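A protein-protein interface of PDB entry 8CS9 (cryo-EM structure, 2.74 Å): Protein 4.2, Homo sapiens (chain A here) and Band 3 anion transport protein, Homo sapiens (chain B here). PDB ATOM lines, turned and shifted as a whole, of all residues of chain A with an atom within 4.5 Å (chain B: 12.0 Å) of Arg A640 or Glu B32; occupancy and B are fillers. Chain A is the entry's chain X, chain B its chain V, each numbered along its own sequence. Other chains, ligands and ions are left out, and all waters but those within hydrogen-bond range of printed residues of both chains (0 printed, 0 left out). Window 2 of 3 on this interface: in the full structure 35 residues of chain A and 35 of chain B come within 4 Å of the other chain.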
ATOM      1  N   CYS A 621      -2.912  -1.859 -14.349  1.00  0.00           N
ATOM      2  CA  CYS A 621      -4.218  -2.451 -14.101  1.00  0.00           C
ATOM      3  C   CYS A 621      -4.077  -3.896 -13.642  1.00  0.00           C
ATOM      4  O   CYS A 621      -3.516  -4.732 -14.357  1.00  0.00           O
ATOM      5  CB  CYS A 621      -5.072  -2.369 -15.360  1.00  0.00           C
ATOM      6  SG  CYS A 621      -5.459  -0.696 -15.896  1.00  0.00           S
ATOM      7  N   PHE A 639      -4.614  -6.754 -16.966  1.00  0.00           N
ATOM      8  CA  PHE A 639      -5.255  -6.415 -18.226  1.00  0.00           C
ATOM      9  C   PHE A 639      -4.692  -5.095 -18.735  1.00  0.00           C
ATOM     10  O   PHE A 639      -4.053  -4.343 -17.994  1.00  0.00           O
ATOM     11  CB  PHE A 639      -6.789  -6.361 -18.095  1.00  0.00           C
ATOM     12  CG  PHE A 639      -7.297  -5.392 -17.064  1.00  0.00           C
ATOM     13  CD1 PHE A 639      -7.427  -5.773 -15.741  1.00  0.00           C
ATOM     14  CD2 PHE A 639      -7.703  -4.120 -17.427  1.00  0.00           C
ATOM     15  CE1 PHE A 639      -7.911  -4.895 -14.792  1.00  0.00           C
ATOM     16  CE2 PHE A 639      -8.191  -3.235 -16.483  1.00  0.00           C
ATOM     17  CZ  PHE A 639      -8.296  -3.624 -15.164  1.00  0.00           C
ATOM     18  N   ARG A 640      -4.920  -4.832 -20.019  1.00  0.00           N
ATOM     19  CA  ARG A 640      -4.266  -3.725 -20.700  1.00  0.00           C
ATOM     20  C   ARG A 640      -4.739  -2.383 -20.148  1.00  0.00           C
ATOM     21  O   ARG A 640      -5.756  -2.284 -19.456  1.00  0.00           O
ATOM     22  CB  ARG A 640      -4.542  -3.781 -22.202  1.00  0.00           C
ATOM     23  CG  ARG A 640      -5.997  -4.030 -22.538  1.00  0.00           C
ATOM     24  CD  ARG A 640      -6.191  -4.417 -23.992  1.00  0.00           C
ATOM     25  NE  ARG A 640      -5.762  -5.785 -24.254  1.00  0.00           N
ATOM     26  CZ  ARG A 640      -4.810  -6.118 -25.115  1.00  0.00           C
ATOM     27  NH1 ARG A 640      -4.171  -5.204 -25.826  1.00  0.00           N
ATOM     28  NH2 ARG A 640      -4.495  -7.400 -25.269  1.00  0.00           N
ATOM     29  N   SER A 641      -3.975  -1.340 -20.464  1.00  0.00           N
ATOM     30  CA  SER A 641      -4.361   0.007 -20.074  1.00  0.00           C
ATOM     31  C   SER A 641      -5.621   0.428 -20.819  1.00  0.00           C
ATOM     32  O   SER A 641      -5.785   0.139 -22.007  1.00  0.00           O
ATOM     33  CB  SER A 641      -3.222   0.986 -20.354  1.00  0.00           C
ATOM     34  OG  SER A 641      -3.622   2.321 -20.103  1.00  0.00           O
ATOM     35  N   VAL A 642      -6.518   1.107 -20.112  1.00  0.00           N
ATOM     36  CA  VAL A 642      -7.819   1.494 -20.645  1.00  0.00           C
ATOM     37  C   VAL A 642      -7.823   3.000 -20.853  1.00  0.00           C
ATOM     38  O   VAL A 642      -7.677   3.767 -19.894  1.00  0.00           O
ATOM     39  CB  VAL A 642      -8.962   1.067 -19.714  1.00  0.00           C
ATOM     40  CG1 VAL A 642     -10.304   1.289 -20.392  1.00  0.00           C
ATOM     41  CG2 VAL A 642      -8.796  -0.384 -19.306  1.00  0.00           C
ATOM     42  N   CYS A 649     -13.267  -5.433 -20.976  1.00  0.00           N
ATOM     43  CA  CYS A 649     -14.178  -6.579 -21.000  1.00  0.00           C
ATOM     44  C   CYS A 649     -13.330  -7.844 -20.849  1.00  0.00           C
ATOM     45  O   CYS A 649     -12.840  -8.396 -21.834  1.00  0.00           O
ATOM     46  CB  CYS A 649     -15.011  -6.604 -22.272  1.00  0.00           C
ATOM     47  SG  CYS A 649     -16.699  -7.200 -22.040  1.00  0.00           S
ATOM     48  N   ALA A 650     -13.191  -8.302 -19.608  1.00  0.00           N
ATOM     49  CA  ALA A 650     -12.379  -9.466 -19.282  1.00  0.00           C
ATOM     50  C   ALA A 650     -13.264 -10.655 -18.945  1.00  0.00           C
ATOM     51  O   ALA A 650     -14.265 -10.519 -18.238  1.00  0.00           O
ATOM     52  CB  ALA A 650     -11.441  -9.164 -18.111  1.00  0.00           C
ATOM     53  N   LYS A 651     -12.893 -11.823 -19.460  1.00  0.00           N
ATOM     54  CA  LYS A 651     -13.613 -13.064 -19.209  1.00  0.00           C
ATOM     55  C   LYS A 651     -12.739 -13.999 -18.388  1.00  0.00           C
ATOM     56  O   LYS A 651     -11.535 -14.111 -18.638  1.00  0.00           O
ATOM     57  CB  LYS A 651     -14.033 -13.736 -20.519  1.00  0.00           C
ATOM     58  CG  LYS A 651     -12.910 -13.899 -21.532  1.00  0.00           C
ATOM     59  CD  LYS A 651     -13.317 -14.796 -22.694  1.00  0.00           C
ATOM     60  CE  LYS A 651     -14.234 -15.924 -22.250  1.00  0.00           C
ATOM     61  NZ  LYS A 651     -14.212 -17.065 -23.206  1.00  0.00           N
ATOM     62  N   GLN B  30     -16.333 -12.401 -22.986  1.00  0.00           N
ATOM     63  CA  GLN B  30     -15.733 -11.081 -23.127  1.00  0.00           C
ATOM     64  C   GLN B  30     -14.546 -11.116 -24.085  1.00  0.00           C
ATOM     65  O   GLN B  30     -14.275 -12.142 -24.711  1.00  0.00           O
ATOM     66  CB  GLN B  30     -15.299 -10.544 -21.765  1.00  0.00           C
ATOM     67  N   MET B  31     -13.831  -9.994 -24.190  1.00  0.00           N
ATOM     68  CA  MET B  31     -12.777  -9.880 -25.193  1.00  0.00           C
ATOM     69  C   MET B  31     -11.383 -10.064 -24.606  1.00  0.00           C
ATOM     70  O   MET B  31     -10.523 -10.668 -25.256  1.00  0.00           O
ATOM     71  CB  MET B  31     -12.870  -8.525 -25.897  1.00  0.00           C
ATOM     72  N   GLU B  32     -11.138  -9.551 -23.403  1.00  0.00           N
ATOM     73  CA  GLU B  32      -9.804  -9.607 -22.817  1.00  0.00           C
ATOM     74  C   GLU B  32      -9.393 -11.039 -22.508  1.00  0.00           C
ATOM     75  O   GLU B  32     -10.200 -11.856 -22.056  1.00  0.00           O
ATOM     76  CB  GLU B  32      -9.753  -8.783 -21.532  1.00  0.00           C
ATOM     77  CG  GLU B  32      -8.379  -8.311 -21.117  1.00  0.00           C
ATOM     78  CD  GLU B  32      -7.905  -7.147 -21.944  1.00  0.00           C
ATOM     79  OE1 GLU B  32      -8.260  -6.002 -21.595  1.00  0.00           O
ATOM     80  OE2 GLU B  32      -7.181  -7.372 -22.935  1.00  0.00           O
ATOM     81  N   GLU B  33      -8.119 -11.340 -22.757  1.00  0.00           N
ATOM     82  CA  GLU B  33      -7.468 -12.558 -22.284  1.00  0.00           C
ATOM     83  C   GLU B  33      -6.451 -12.112 -21.243  1.00  0.00           C
ATOM     84  O   GLU B  33      -5.261 -11.948 -21.555  1.00  0.00           O
ATOM     85  CB  GLU B  33      -6.808 -13.337 -23.422  1.00  0.00           C
ATOM     86  CG  GLU B  33      -7.723 -14.319 -24.160  1.00  0.00           C
ATOM     87  CD  GLU B  33      -8.654 -15.107 -23.249  1.00  0.00           C
ATOM     88  OE1 GLU B  33      -8.219 -15.563 -22.170  1.00  0.00           O
ATOM     89  OE2 GLU B  33      -9.833 -15.279 -23.624  1.00  0.00           O
ATOM     90  N   PRO B  34      -6.885 -11.886 -20.002  1.00  0.00           N
ATOM     91  CA  PRO B  34      -5.994 -11.281 -19.006  1.00  0.00           C
ATOM     92  C   PRO B  34      -4.820 -12.188 -18.664  1.00  0.00           C
ATOM     93  O   PRO B  34      -4.969 -13.400 -18.503  1.00  0.00           O
ATOM     94  CB  PRO B  34      -6.916 -11.063 -17.802  1.00  0.00           C
ATOM     95  CG  PRO B  34      -7.982 -12.090 -17.967  1.00  0.00           C
ATOM     96  CD  PRO B  34      -8.214 -12.181 -19.442  1.00  0.00           C
ATOM     97  N   ALA B  35      -3.646 -11.577 -18.546  1.00  0.00           N
ATOM     98  CA  ALA B  35      -2.416 -12.301 -18.265  1.00  0.00           C
ATOM     99  C   ALA B  35      -2.225 -12.423 -16.760  1.00  0.00           C
ATOM    100  O   ALA B  35      -2.473 -11.466 -16.021  1.00  0.00           O
ATOM    101  CB  ALA B  35      -1.218 -11.593 -18.897  1.00  0.00           C
ATOM    102  N   ALA B  36      -1.782 -13.597 -16.318  1.00  0.00           N
ATOM    103  CA  ALA B  36      -1.625 -13.864 -14.896  1.00  0.00           C
ATOM    104  C   ALA B  36      -0.592 -12.932 -14.276  1.00  0.00           C
ATOM    105  O   ALA B  36       0.436 -12.622 -14.882  1.00  0.00           O
ATOM    106  CB  ALA B  36      -1.212 -15.319 -14.676  1.00  0.00           C
ATOM    107  N   HIS B  37      -0.884 -12.479 -13.063  1.00  0.00           N
ATOM    108  CA  HIS B  37      -0.004 -11.605 -12.295  1.00  0.00           C
ATOM    109  C   HIS B  37       0.426 -12.358 -11.043  1.00  0.00           C
ATOM    110  O   HIS B  37      -0.388 -12.597 -10.145  1.00  0.00           O
ATOM    111  CB  HIS B  37      -0.707 -10.296 -11.948  1.00  0.00           C
ATOM    112  CG  HIS B  37       0.231  -9.196 -11.597  1.00  0.00           C
ATOM    113  ND1 HIS B  37      -0.054  -8.251 -10.637  1.00  0.00           N
ATOM    114  CD2 HIS B  37       1.469  -8.912 -12.054  1.00  0.00           C
ATOM    115  CE1 HIS B  37       0.966  -7.425 -10.524  1.00  0.00           C
ATOM    116  NE2 HIS B  37       1.916  -7.826 -11.349  1.00  0.00           N
ATOM    117  N   ILE B 140      -3.453 -23.937 -15.306  1.00  0.00           N
ATOM    118  CA  ILE B 140      -3.674 -22.951 -16.358  1.00  0.00           C
ATOM    119  C   ILE B 140      -3.214 -21.571 -15.905  1.00  0.00           C
ATOM    120  O   ILE B 140      -2.610 -20.818 -16.680  1.00  0.00           O
ATOM    121  CB  ILE B 140      -5.153 -22.953 -16.784  1.00  0.00           C
ATOM    122  CG1 ILE B 140      -5.416 -24.105 -17.747  1.00  0.00           C
ATOM    123  CG2 ILE B 140      -5.551 -21.636 -17.425  1.00  0.00           C
ATOM    124  CD1 ILE B 140      -6.852 -24.470 -17.848  1.00  0.00           C
ATOM    125  N   PRO B 147      -4.849 -24.146 -22.123  1.00  0.00           N
ATOM    126  CA  PRO B 147      -6.277 -24.412 -21.888  1.00  0.00           C
ATOM    127  C   PRO B 147      -6.848 -25.540 -22.732  1.00  0.00           C
ATOM    128  O   PRO B 147      -7.873 -26.118 -22.353  1.00  0.00           O
ATOM    129  CB  PRO B 147      -6.939 -23.068 -22.222  1.00  0.00           C
ATOM    130  CG  PRO B 147      -5.879 -22.061 -22.006  1.00  0.00           C
ATOM    131  CD  PRO B 147      -4.589 -22.720 -22.386  1.00  0.00           C
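NE of Arg A640 is in salt-bridge range of OE2 of Glu B32 (2.5 Å).
The backbone NH of Met B31 sits at hydrogen-bond distance from the backbone carbonyl oxygen of Cys A649, 3.0 Å away.
O of Cys A649 sits at hydrogen-bond distance from N of Glu B32, 2.6 Å away.
The backbone carbonyl oxygen (O) of Cys A621 is in hydrogen-bond range of the backbone NH (N) of Phe A639 (3.5 Å).
Of chain B, only Glu B32 (3.8 Å) comes within 4 Å of Phe A639.
Arg A640 touches just one residue of chain B: Glu B32.
Of chain B, only Gln B30 (3.3 Å), Met B31 (3.0 Å) and Glu B32 (2.6 Å) come within 4 Å of Cys A649.
Ala A650 touches two residues of chain B.
Of chain B, only Gln B30, Glu B32, Glu B33 and Pro B34 come within 4 Å of Lys A651.
Of the printed residues of chain A, Met B31 touches Cys A649.
Of chain A, only Phe A639, Arg A640, Cys A649, Ala A650 and Lys A651 come within 4 Å of Glu B32.
Of the printed residues of chain A, Pro B34 touches Lys A651.
Ala B35 touches none of the printed residues of chain A.
Pro B147 touches none of the printed residues of chain A.
The nearest residue of chain B that does not touch Arg A640 is Glu B33 (5.9 Å).
The nearest printed residue of chain A that does not touch Pro B34 is Ala A650 (4.5 Å).
Hydrophobic or aromatic side chains of chain B within 4 Å of the printed part of chain A: Pro B34.
Among the printed residues, 11 pairs touch across the chains.
Among the printed residues, Asp or Glu carboxylates within 4 Å of a Lys or Arg side-chain nitrogen of the other chain: Arg A640 with Glu B32 (2.5 Å).
Among the printed residues, pairs that only touch across the chains: Phe A639 with Glu B32 (3.8 Å), Cys A649 with Gln B30 (3.3 Å), Ala A650 with Gln B30 (3.5 Å), Ala A650 with Glu B32 (3.5 Å), Lys A651 with Gln B30 (3.5 Å), Lys A651 with Glu B32 (3.4 Å), Lys A651 with Glu B33 (3.6 Å) and Lys A651 with Pro B34 (3.9 Å).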
